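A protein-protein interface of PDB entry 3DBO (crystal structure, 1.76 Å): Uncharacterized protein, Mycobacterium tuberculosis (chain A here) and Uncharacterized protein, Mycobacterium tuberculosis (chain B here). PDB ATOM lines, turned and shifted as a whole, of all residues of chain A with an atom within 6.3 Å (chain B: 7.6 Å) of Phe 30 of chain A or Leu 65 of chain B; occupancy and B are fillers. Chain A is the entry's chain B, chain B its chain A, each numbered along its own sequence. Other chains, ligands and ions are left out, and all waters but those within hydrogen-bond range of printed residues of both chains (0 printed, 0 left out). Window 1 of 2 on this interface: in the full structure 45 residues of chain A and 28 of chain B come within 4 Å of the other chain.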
ATOM      1  N   LEU A  25     -30.904  22.352   4.486  1.00  0.00           N
ATOM      2  CA  LEU A  25     -29.534  21.983   4.833  1.00  0.00           C
ATOM      3  C   LEU A  25     -29.325  22.076   6.334  1.00  0.00           C
ATOM      4  O   LEU A  25     -29.781  23.038   6.954  1.00  0.00           O
ATOM      5  CB  LEU A  25     -28.547  22.930   4.131  1.00  0.00           C
ATOM      6  CG  LEU A  25     -28.798  23.107   2.632  1.00  0.00           C
ATOM      7  CD1 LEU A  25     -28.012  24.312   2.105  1.00  0.00           C
ATOM      8  CD2 LEU A  25     -28.435  21.796   1.892  1.00  0.00           C
ATOM      9  N   ASP A  26     -28.660  21.074   6.905  1.00  0.00           N
ATOM     10  CA  ASP A  26     -28.246  21.121   8.302  1.00  0.00           C
ATOM     11  C   ASP A  26     -26.859  21.754   8.364  1.00  0.00           C
ATOM     12  O   ASP A  26     -26.339  22.191   7.328  1.00  0.00           O
ATOM     13  CB  ASP A  26     -28.280  19.725   8.922  1.00  0.00           C
ATOM     14  CG  ASP A  26     -27.046  18.889   8.578  1.00  0.00           C
ATOM     15  OD1 ASP A  26     -26.410  19.154   7.537  1.00  0.00           O
ATOM     16  OD2 ASP A  26     -26.698  17.995   9.377  1.00  0.00           O
ATOM     17  N   THR A  27     -26.227  21.771   9.535  1.00  0.00           N
ATOM     18  CA  THR A  27     -24.911  22.407   9.652  1.00  0.00           C
ATOM     19  C   THR A  27     -23.784  21.611   8.982  1.00  0.00           C
ATOM     20  O   THR A  27     -22.867  22.200   8.410  1.00  0.00           O
ATOM     21  CB  THR A  27     -24.580  22.707  11.128  1.00  0.00           C
ATOM     22  OG1 THR A  27     -25.691  23.425  11.698  1.00  0.00           O
ATOM     23  CG2 THR A  27     -23.342  23.552  11.234  1.00  0.00           C
ATOM     24  N   SER A  28     -23.868  20.277   9.045  1.00  0.00           N
ATOM     25  CA  SER A  28     -22.816  19.398   8.536  1.00  0.00           C
ATOM     26  C   SER A  28     -22.502  19.563   7.039  1.00  0.00           C
ATOM     27  O   SER A  28     -21.349  19.394   6.622  1.00  0.00           O
ATOM     28  CB  SER A  28     -23.140  17.924   8.874  1.00  0.00           C
ATOM     29  OG  SER A  28     -24.189  17.448   8.058  1.00  0.00           O
ATOM     30  N   VAL A  29     -23.494  19.930   6.234  1.00  0.00           N
ATOM     31  CA  VAL A  29     -23.266  20.166   4.795  1.00  0.00           C
ATOM     32  C   VAL A  29     -22.281  21.337   4.566  1.00  0.00           C
ATOM     33  O   VAL A  29     -21.552  21.360   3.563  1.00  0.00           O
ATOM     34  CB  VAL A  29     -24.572  20.379   3.965  1.00  0.00           C
ATOM     35  CG1 VAL A  29     -25.479  19.158   4.049  1.00  0.00           C
ATOM     36  CG2 VAL A  29     -25.314  21.640   4.394  1.00  0.00           C
ATOM     37  N   PHE A  30     -22.267  22.307   5.492  1.00  0.00           N
ATOM     38  CA  PHE A  30     -21.393  23.483   5.376  1.00  0.00           C
ATOM     39  C   PHE A  30     -19.945  23.185   5.783  1.00  0.00           C
ATOM     40  O   PHE A  30     -19.037  23.969   5.492  1.00  0.00           O
ATOM     41  CB  PHE A  30     -21.946  24.678   6.205  1.00  0.00           C
ATOM     42  CG  PHE A  30     -23.200  25.245   5.664  1.00  0.00           C
ATOM     43  CD1 PHE A  30     -23.163  26.290   4.743  1.00  0.00           C
ATOM     44  CD2 PHE A  30     -24.448  24.735   6.057  1.00  0.00           C
ATOM     45  CE1 PHE A  30     -24.330  26.812   4.224  1.00  0.00           C
ATOM     46  CE2 PHE A  30     -25.610  25.243   5.537  1.00  0.00           C
ATOM     47  CZ  PHE A  30     -25.577  26.293   4.620  1.00  0.00           C
ATOM     48  N   ILE A  31     -19.726  22.053   6.440  1.00  0.00           N
ATOM     49  CA  ILE A  31     -18.412  21.681   6.952  1.00  0.00           C
ATOM     50  C   ILE A  31     -17.688  20.685   6.023  1.00  0.00           C
ATOM     51  O   ILE A  31     -18.318  19.792   5.459  1.00  0.00           O
ATOM     52  CB  ILE A  31     -18.522  21.119   8.386  1.00  0.00           C
ATOM     53  CG1 ILE A  31     -19.343  22.070   9.270  1.00  0.00           C
ATOM     54  CG2 ILE A  31     -17.131  20.890   8.994  1.00  0.00           C
ATOM     55  CD1 ILE A  31     -19.633  21.540  10.679  1.00  0.00           C
ATOM     56  N   ALA A  32     -16.378  20.862   5.839  1.00  0.00           N
ATOM     57  CA  ALA A  32     -15.565  19.887   5.065  1.00  0.00           C
ATOM     58  C   ALA A  32     -15.424  18.557   5.822  1.00  0.00           C
ATOM     59  O   ALA A  32     -15.205  18.547   7.047  1.00  0.00           O
ATOM     60  CB  ALA A  32     -14.164  20.463   4.728  1.00  0.00           C
ATOM     61  N   LEU A  39     -19.455  16.600  -1.371  1.00  0.00           N
ATOM     62  CA  LEU A  39     -20.842  16.201  -1.138  1.00  0.00           C
ATOM     63  C   LEU A  39     -21.398  15.434  -2.324  1.00  0.00           C
ATOM     64  O   LEU A  39     -20.904  15.566  -3.451  1.00  0.00           O
ATOM     65  CB  LEU A  39     -21.736  17.419  -0.856  1.00  0.00           C
ATOM     66  CG  LEU A  39     -21.285  18.363   0.258  1.00  0.00           C
ATOM     67  CD1 LEU A  39     -22.165  19.593   0.282  1.00  0.00           C
ATOM     68  CD2 LEU A  39     -21.288  17.658   1.613  1.00  0.00           C
ATOM     69  N   ALA A  49     -32.800  25.698   1.437  1.00  0.00           N
ATOM     70  CA  ALA A  49     -32.796  26.700   2.517  1.00  0.00           C
ATOM     71  C   ALA A  49     -32.002  26.111   3.687  1.00  0.00           C
ATOM     72  O   ALA A  49     -31.611  24.939   3.659  1.00  0.00           O
ATOM     73  CB  ALA A  49     -34.228  27.035   2.957  1.00  0.00           C
ATOM     74  N   THR A  50     -31.737  26.908   4.723  1.00  0.00           N
ATOM     75  CA  THR A  50     -31.239  26.313   5.949  1.00  0.00           C
ATOM     76  C   THR A  50     -32.122  26.824   7.101  1.00  0.00           C
ATOM     77  O   THR A  50     -33.222  27.366   6.852  1.00  0.00           O
ATOM     78  CB  THR A  50     -29.723  26.568   6.139  1.00  0.00           C
ATOM     79  OG1 THR A  50     -29.229  25.786   7.230  1.00  0.00           O
ATOM     80  CG2 THR A  50     -29.403  28.083   6.346  1.00  0.00           C
ATOM     81  N   THR A  54     -28.596  26.460  12.174  1.00  0.00           N
ATOM     82  CA  THR A  54     -27.322  26.454  11.440  1.00  0.00           C
ATOM     83  C   THR A  54     -26.707  27.844  11.425  1.00  0.00           C
ATOM     84  O   THR A  54     -25.490  27.966  11.588  1.00  0.00           O
ATOM     85  CB  THR A  54     -27.485  25.900  10.016  1.00  0.00           C
ATOM     86  OG1 THR A  54     -27.810  24.507  10.107  1.00  0.00           O
ATOM     87  CG2 THR A  54     -26.183  26.071   9.187  1.00  0.00           C
ATOM     88  N   LEU A  58     -22.914  28.104  12.829  1.00  0.00           N
ATOM     89  CA  LEU A  58     -21.835  28.695  12.001  1.00  0.00           C
ATOM     90  C   LEU A  58     -21.269  29.957  12.666  1.00  0.00           C
ATOM     91  O   LEU A  58     -20.063  30.192  12.640  1.00  0.00           O
ATOM     92  CB  LEU A  58     -22.332  28.978  10.580  1.00  0.00           C
ATOM     93  CG  LEU A  58     -22.748  27.736   9.765  1.00  0.00           C
ATOM     94  CD1 LEU A  58     -23.233  28.197   8.410  1.00  0.00           C
ATOM     95  CD2 LEU A  58     -21.568  26.755   9.660  1.00  0.00           C
ATOM     96  N   THR A  77     -17.730  30.638   5.610  1.00  0.00           N
ATOM     97  CA  THR A  77     -18.853  29.679   5.723  1.00  0.00           C
ATOM     98  C   THR A  77     -20.122  30.415   6.200  1.00  0.00           C
ATOM     99  O   THR A  77     -21.213  30.245   5.638  1.00  0.00           O
ATOM    100  CB  THR A  77     -18.494  28.527   6.688  1.00  0.00           C
ATOM    101  OG1 THR A  77     -17.178  28.036   6.381  1.00  0.00           O
ATOM    102  CG2 THR A  77     -19.510  27.389   6.567  1.00  0.00           C
ATOM    103  N   SER A  80     -21.666  32.470   3.532  1.00  0.00           N
ATOM    104  CA  SER A  80     -22.306  31.699   2.443  1.00  0.00           C
ATOM    105  C   SER A  80     -23.825  31.562   2.612  1.00  0.00           C
ATOM    106  O   SER A  80     -24.533  31.276   1.648  1.00  0.00           O
ATOM    107  CB  SER A  80     -21.637  30.325   2.242  1.00  0.00           C
ATOM    108  OG  SER A  80     -22.072  29.358   3.186  1.00  0.00           O
ATOM    109  N   VAL A  81     -24.323  31.781   3.828  1.00  0.00           N
ATOM    110  CA  VAL A  81     -25.776  31.748   4.032  1.00  0.00           C
ATOM    111  C   VAL A  81     -26.460  33.104   3.990  1.00  0.00           C
ATOM    112  O   VAL A  81     -27.661  33.186   4.233  1.00  0.00           O
ATOM    113  CB  VAL A  81     -26.171  30.972   5.293  1.00  0.00           C
ATOM    114  CG1 VAL A  81     -25.670  29.561   5.171  1.00  0.00           C
ATOM    115  CG2 VAL A  81     -25.613  31.610   6.540  1.00  0.00           C
ATOM    116  N   MET A  84     -29.345  33.216   1.629  1.00  0.00           N
ATOM    117  CA  MET A  84     -30.153  31.996   1.677  1.00  0.00           C
ATOM    118  C   MET A  84     -31.267  32.135   2.710  1.00  0.00           C
ATOM    119  O   MET A  84     -31.041  32.672   3.796  1.00  0.00           O
ATOM    120  CB  MET A  84     -29.236  30.804   1.999  1.00  0.00           C
ATOM    121  CG  MET A  84     -29.918  29.428   2.084  1.00  0.00           C
ATOM    122  SD  MET A  84     -28.868  28.061   2.639  1.00  0.00           S
ATOM    123  CE  MET A  84     -27.554  28.103   1.410  1.00  0.00           C
ATOM    124  N   GLN A 132     -24.853  15.728   5.861  1.00  0.00           N
ATOM    125  CA  GLN A 132     -23.640  15.018   5.522  1.00  0.00           C
ATOM    126  C   GLN A 132     -23.293  14.020   6.622  1.00  0.00           C
ATOM    127  O   GLN A 132     -22.526  13.095   6.384  1.00  0.00           O
ATOM    128  CB  GLN A 132     -22.478  16.005   5.264  1.00  0.00           C
ATOM    129  CG  GLN A 132     -21.234  15.329   4.775  1.00  0.00           C
ATOM    130  CD  GLN A 132     -20.045  16.248   4.585  1.00  0.00           C
ATOM    131  OE1 GLN A 132     -19.083  15.858   3.936  1.00  0.00           O
ATOM    132  NE2 GLN A 132     -20.094  17.468   5.140  1.00  0.00           N
ATOM    133  N   LEU B  56     -32.226  29.306  -2.511  1.00  0.00           N
ATOM    134  CA  LEU B  56     -31.149  29.185  -3.488  1.00  0.00           C
ATOM    135  C   LEU B  56     -31.352  27.962  -4.372  1.00  0.00           C
ATOM    136  O   LEU B  56     -31.790  26.909  -3.902  1.00  0.00           O
ATOM    137  CB  LEU B  56     -29.788  29.086  -2.786  1.00  0.00           C
ATOM    138  CG  LEU B  56     -28.893  30.316  -2.582  1.00  0.00           C
ATOM    139  CD1 LEU B  56     -29.616  31.471  -1.926  1.00  0.00           C
ATOM    140  CD2 LEU B  56     -27.671  29.941  -1.766  1.00  0.00           C
ATOM    141  N   THR B  59     -27.390  25.003  -7.932  1.00  0.00           N
ATOM    142  CA  THR B  59     -26.150  25.531  -8.508  1.00  0.00           C
ATOM    143  C   THR B  59     -25.680  26.775  -7.763  1.00  0.00           C
ATOM    144  O   THR B  59     -24.494  26.904  -7.460  1.00  0.00           O
ATOM    145  CB  THR B  59     -26.289  25.849 -10.013  1.00  0.00           C
ATOM    146  OG1 THR B  59     -27.314  25.025 -10.584  1.00  0.00           O
ATOM    147  CG2 THR B  59     -24.959  25.595 -10.730  1.00  0.00           C
ATOM    148  N   GLU B  60     -26.621  27.679  -7.481  1.00  0.00           N
ATOM    149  CA  GLU B  60     -26.364  28.865  -6.659  1.00  0.00           C
ATOM    150  C   GLU B  60     -25.715  28.481  -5.323  1.00  0.00           C
ATOM    151  O   GLU B  60     -24.604  28.929  -5.020  1.00  0.00           O
ATOM    152  CB  GLU B  60     -27.660  29.647  -6.415  1.00  0.00           C
ATOM    153  CG  GLU B  60     -28.087  30.556  -7.560  1.00  0.00           C
ATOM    154  CD  GLU B  60     -29.371  31.313  -7.258  1.00  0.00           C
ATOM    155  OE1 GLU B  60     -30.334  30.693  -6.755  1.00  0.00           O
ATOM    156  OE2 GLU B  60     -29.421  32.529  -7.529  1.00  0.00           O
ATOM    157  N   PHE B  61     -26.396  27.639  -4.539  1.00  0.00           N
ATOM    158  CA  PHE B  61     -25.854  27.177  -3.257  1.00  0.00           C
ATOM    159  C   PHE B  61     -24.443  26.628  -3.413  1.00  0.00           C
ATOM    160  O   PHE B  61     -23.518  27.088  -2.740  1.00  0.00           O
ATOM    161  CB  PHE B  61     -26.760  26.124  -2.599  1.00  0.00           C
ATOM    162  CG  PHE B  61     -26.045  25.254  -1.584  1.00  0.00           C
ATOM    163  CD1 PHE B  61     -25.497  25.812  -0.420  1.00  0.00           C
ATOM    164  CD2 PHE B  61     -25.913  23.882  -1.793  1.00  0.00           C
ATOM    165  CE1 PHE B  61     -24.824  25.020   0.512  1.00  0.00           C
ATOM    166  CE2 PHE B  61     -25.244  23.074  -0.859  1.00  0.00           C
ATOM    167  CZ  PHE B  61     -24.702  23.649   0.295  1.00  0.00           C
ATOM    168  N   LEU B  62     -24.290  25.645  -4.300  1.00  0.00           N
ATOM    169  CA  LEU B  62     -23.003  24.986  -4.518  1.00  0.00           C
ATOM    170  C   LEU B  62     -21.923  25.955  -4.993  1.00  0.00           C
ATOM    171  O   LEU B  62     -20.740  25.731  -4.746  1.00  0.00           O
ATOM    172  CB  LEU B  62     -23.137  23.801  -5.483  1.00  0.00           C
ATOM    173  CG  LEU B  62     -23.812  22.528  -4.954  1.00  0.00           C
ATOM    174  CD1 LEU B  62     -24.028  21.541  -6.081  1.00  0.00           C
ATOM    175  CD2 LEU B  62     -23.025  21.885  -3.818  1.00  0.00           C
ATOM    176  N   SER B  63     -22.336  27.039  -5.656  1.00  0.00           N
ATOM    177  CA  SER B  63     -21.406  28.114  -6.011  1.00  0.00           C
ATOM    178  C   SER B  63     -20.980  28.930  -4.787  1.00  0.00           C
ATOM    179  O   SER B  63     -19.803  29.286  -4.663  1.00  0.00           O
ATOM    180  CB  SER B  63     -21.994  29.033  -7.087  1.00  0.00           C
ATOM    181  OG  SER B  63     -21.991  28.388  -8.346  1.00  0.00           O
ATOM    182  N   ARG B  64     -21.933  29.228  -3.898  1.00  0.00           N
ATOM    183  CA  ARG B  64     -21.642  29.994  -2.676  1.00  0.00           C
ATOM    184  C   ARG B  64     -20.811  29.174  -1.685  1.00  0.00           C
ATOM    185  O   ARG B  64     -20.008  29.728  -0.931  1.00  0.00           O
ATOM    186  CB  ARG B  64     -22.930  30.473  -1.983  1.00  0.00           C
ATOM    187  CG  ARG B  64     -24.054  30.955  -2.904  1.00  0.00           C
ATOM    188  CD  ARG B  64     -23.650  32.134  -3.783  1.00  0.00           C
ATOM    189  NE  ARG B  64     -24.372  32.124  -5.055  1.00  0.00           N
ATOM    190  CZ  ARG B  64     -25.538  32.727  -5.260  1.00  0.00           C
ATOM    191  NH1 ARG B  64     -26.119  33.401  -4.275  1.00  0.00           N
ATOM    192  NH2 ARG B  64     -26.120  32.660  -6.450  1.00  0.00           N
ATOM    193  N   LEU B  65     -21.011  27.858  -1.701  1.00  0.00           N
ATOM    194  CA  LEU B  65     -20.365  26.962  -0.740  1.00  0.00           C
ATOM    195  C   LEU B  65     -18.969  26.516  -1.156  1.00  0.00           C
ATOM    196  O   LEU B  65     -18.102  26.320  -0.302  1.00  0.00           O
ATOM    197  CB  LEU B  65     -21.242  25.726  -0.468  1.00  0.00           C
ATOM    198  CG  LEU B  65     -20.650  24.688   0.499  1.00  0.00           C
ATOM    199  CD1 LEU B  65     -20.776  25.146   1.946  1.00  0.00           C
ATOM    200  CD2 LEU B  65     -21.267  23.314   0.304  1.00  0.00           C
ATOM    201  N   ARG B  66     -18.751  26.319  -2.455  1.00  0.00           N
ATOM    202  CA  ARG B  66     -17.460  25.775  -2.899  1.00  0.00           C
ATOM    203  C   ARG B  66     -16.337  26.774  -2.691  1.00  0.00           C
ATOM    204  O   ARG B  66     -16.397  27.908  -3.171  1.00  0.00           O
ATOM    205  CB  ARG B  66     -17.514  25.212  -4.326  1.00  0.00           C
ATOM    206  CG  ARG B  66     -18.366  23.947  -4.404  1.00  0.00           C
ATOM    207  CD  ARG B  66     -17.722  22.834  -5.202  1.00  0.00           C
ATOM    208  NE  ARG B  66     -18.194  21.531  -4.736  1.00  0.00           N
ATOM    209  CZ  ARG B  66     -18.902  21.349  -3.625  1.00  0.00           C
ATOM    210  NH1 ARG B  66     -19.217  22.387  -2.860  1.00  0.00           N
ATOM    211  NH2 ARG B  66     -19.292  20.132  -3.272  1.00  0.00           N
ATOM    212  N   GLY B  67     -15.332  26.345  -1.934  1.00  0.00           N
ATOM    213  CA  GLY B  67     -14.275  27.233  -1.460  1.00  0.00           C
ATOM    214  C   GLY B  67     -14.596  27.926  -0.142  1.00  0.00           C
ATOM    215  O   GLY B  67     -13.759  28.667   0.388  1.00  0.00           O
ATOM    216  N   ALA B  68     -15.800  27.693   0.387  1.00  0.00           N
ATOM    217  CA  ALA B  68     -16.242  28.336   1.631  1.00  0.00           C
ATOM    218  C   ALA B  68     -16.651  27.346   2.734  1.00  0.00           C
ATOM    219  O   ALA B  68     -17.233  27.748   3.735  1.00  0.00           O
ATOM    220  CB  ALA B  68     -17.379  29.330   1.351  1.00  0.00           C
ATOM    221  N   GLN B  69     -16.336  26.063   2.562  1.00  0.00           N
ATOM    222  CA  GLN B  69     -16.618  25.062   3.600  1.00  0.00           C
ATOM    223  C   GLN B  69     -15.799  25.320   4.860  1.00  0.00           C
ATOM    224  O   GLN B  69     -14.640  25.722   4.793  1.00  0.00           O
ATOM    225  CB  GLN B  69     -16.383  23.634   3.093  1.00  0.00           C
ATOM    226  CG  GLN B  69     -17.556  23.055   2.302  1.00  0.00           C
ATOM    227  CD  GLN B  69     -17.649  21.533   2.401  1.00  0.00           C
ATOM    228  OE1 GLN B  69     -16.644  20.821   2.281  1.00  0.00           O
ATOM    229  NE2 GLN B  69     -18.859  21.031   2.619  1.00  0.00           N
ATOM    230  N   ALA B  70     -16.415  25.110   6.011  1.00  0.00           N
ATOM    231  CA  ALA B  70     -15.715  25.264   7.278  1.00  0.00           C
ATOM    232  C   ALA B  70     -14.669  24.157   7.390  1.00  0.00           C
ATOM    233  O   ALA B  70     -14.792  23.111   6.742  1.00  0.00           O
ATOM    234  CB  ALA B  70     -16.702  25.196   8.429  1.00  0.00           C
ATOM    235  N   ASP B  71     -13.633  24.399   8.185  1.00  0.00           N
ATOM    236  CA  ASP B  71     -12.646  23.370   8.508  1.00  0.00           C
ATOM    237  C   ASP B  71     -13.326  22.192   9.220  1.00  0.00           C
ATOM    238  O   ASP B  71     -14.292  22.391   9.969  1.00  0.00           O
ATOM    239  CB  ASP B  71     -11.570  23.957   9.422  1.00  0.00           C
ATOM    240  CG  ASP B  71     -12.151  24.531  10.712  1.00  0.00           C
ATOM    241  OD1 ASP B  71     -12.956  25.488  10.624  1.00  0.00           O
ATOM    242  OD2 ASP B  71     -11.803  24.033  11.804  1.00  0.00           O
ATOM    243  N   LEU B  74     -14.498  22.241  12.925  1.00  0.00           N
ATOM    244  CA  LEU B  74     -15.763  22.818  13.411  1.00  0.00           C
ATOM    245  C   LEU B  74     -16.671  21.746  14.019  1.00  0.00           C
ATOM    246  O   LEU B  74     -17.445  22.032  14.937  1.00  0.00           O
ATOM    247  CB  LEU B  74     -16.499  23.610  12.325  1.00  0.00           C
ATOM    248  CG  LEU B  74     -17.754  24.400  12.745  1.00  0.00           C
ATOM    249  CD1 LEU B  74     -17.459  25.371  13.873  1.00  0.00           C
ATOM    250  CD2 LEU B  74     -18.388  25.130  11.564  1.00  0.00           C
ATOM    251  N   ARG B  75     -16.567  20.512  13.516  1.00  0.00           N
ATOM    252  CA  ARG B  75     -17.307  19.386  14.106  1.00  0.00           C
ATOM    253  C   ARG B  75     -16.927  19.189  15.556  1.00  0.00           C
ATOM    254  O   ARG B  75     -17.790  18.926  16.389  1.00  0.00           O
ATOM    255  CB  ARG B  75     -17.065  18.086  13.346  1.00  0.00           C
ATOM    256  CG  ARG B  75     -17.750  18.059  12.020  1.00  0.00           C
ATOM    257  CD  ARG B  75     -17.883  16.643  11.463  1.00  0.00           C
ATOM    258  NE  ARG B  75     -18.677  16.703  10.238  1.00  0.00           N
ATOM    259  CZ  ARG B  75     -18.188  17.036   9.046  1.00  0.00           C
ATOM    260  NH1 ARG B  75     -16.896  17.321   8.913  1.00  0.00           N
ATOM    261  NH2 ARG B  75     -18.987  17.082   7.986  1.00  0.00           N
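NE2 of Gln 69 of chain B is in hydrogen-bond range of O of Val 29 of chain A (2.9 Å). The side-chain hydroxyl (OG1) of Thr 77 of chain A sits at hydrogen-bond distance from the backbone NH (N) of Ala 70 of chain B (3.0 Å). The backbone carbonyl oxygen (O) of Phe 30 of chain A sits at hydrogen-bond distance from the backbone NH (N) of Ala 70 of chain B (2.9 Å). The backbone carbonyl oxygen of Ala 70 of chain B is in hydrogen-bond range of the backbone NH of Ala 32 of chain A, at 2.9 Å. OG1 of Thr 77 of chain A sits at hydrogen-bond distance from O of Ala 68 of chain B. The guanidinium group (NH2) of Arg 75 of chain B sits close to the side-chain amide nitrogen (NE2) of Gln 132 of chain A, at 3.1 Å. O of Ile 31 of chain A sits at hydrogen-bond distance from NE2 of Gln 69 of chain B (3.1 Å). The guanidinium group of Arg 75 of chain B sits at hydrogen-bond distance from the backbone carbonyl oxygen of Ala 32 of chain A.
The backbone NH (N) of Leu 74 of chain B lies within hydrogen-bond range of the side-chain carboxylate (OD2) of Asp 71 of chain B (3.4 Å). The backbone carbonyl oxygen (O) of Thr 77 of chain A is in hydrogen-bond range of the side-chain hydroxyl (OG) of Ser 80 of chain A (2.7 Å). The side-chain carboxylate of Asp 26 of chain A sits at hydrogen-bond distance from the backbone NH of Val 29 of chain A (3.3 Å). The side-chain carboxylate of Asp 26 of chain A lies within hydrogen-bond range of the side-chain hydroxyl of Ser 28 of chain A, at 2.8 Å. The backbone carbonyl oxygen (O) of Ser 28 of chain A lies within hydrogen-bond range of the side-chain amide nitrogen (NE2) of Gln 132 of chain A (2.7 Å). OG1 of Thr 50 of chain A lies within hydrogen-bond range of O of Leu 25 of chain A (2.8 Å).
Among the printed residues, pairs that only touch across the chains: Ala 32 of chain A with Gln 69 of chain B (3.1 Å), Phe 30 of chain A with Gln 69 of chain B (3.3 Å), Ile 31 of chain A with Asp 71 of chain B (3.4 Å), Thr 77 of chain A with Gln 69 of chain B (3.4 Å), Ser 28 of chain A with Arg 75 of chain B (3.6 Å), Ile 31 of chain A with Arg 75 of chain B (3.6 Å), Met 84 of chain A with Phe 61 of chain B (3.6 Å), Ser 80 of chain A with Arg 64 of chain B (3.6 Å), Leu 25 of chain A with Phe 61 of chain B (3.6 Å), Met 84 of chain A with Leu 56 of chain B (3.7 Å), Val 29 of chain A with Leu 65 of chain B (3.8 Å), Leu 39 of chain A with Leu 65 of chain B (3.8 Å), Ile 31 of chain A with Ala 70 of chain B (3.8 Å), Phe 30 of chain A with Leu 65 of chain B (3.9 Å) and Ile 31 of chain A with Leu 74 of chain B (3.9 Å).
Of chain B, only Leu 65, Gln 69 and Ala 70 come within 4 Å of Phe 30 of chain A. Of the printed residues of chain B, Ile 31 of chain A touches Gln 69, Ala 70, Asp 71, Leu 74 and Arg 75. Printed residues of chain B within 4 Å of Ala 32 of chain A: Gln 69 (3.1 Å), Ala 70 (2.9 Å) and Arg 75 (2.8 Å). Thr 54 of chain A touches none of the printed residues of chain B. Of the printed residues of chain B, Ser 80 of chain A touches Arg 64 (3.6 Å). Thr 59 of chain B touches none of the printed residues of chain A. Of the printed residues of chain A, Leu 65 of chain B touches Val 29 (3.8 Å), Phe 30 (3.9 Å) and Leu 39 (3.8 Å). Of the printed residues of chain A, Leu 74 of chain B touches Ile 31. Of the printed residues of chain A, Arg 75 of chain B touches Ser 28 (3.6 Å), Ile 31 (3.6 Å), Ala 32 (2.8 Å) and Gln 132 (3.1 Å). The nearest printed residue of chain A that does not touch Leu 65 of chain B is Ser 80 of chain A (4.6 Å).
Printed residues of chain B that touch a printed residue of chain A: Leu 56, Phe 61, Arg 64, Leu 65, Ala 68, Gln 69, Ala 70, Asp 71, Leu 74 and Arg 75. Of the 18 printed residues of chain A, 11 touch a printed residue of chain B. Hydrophobic or aromatic side chains of chain A that line the printed part of chain B: Leu 25, Phe 30, Ile 31, Ala 32, Leu 39 and Met 84. Among the printed residues, 23 pairs touch across the chains.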
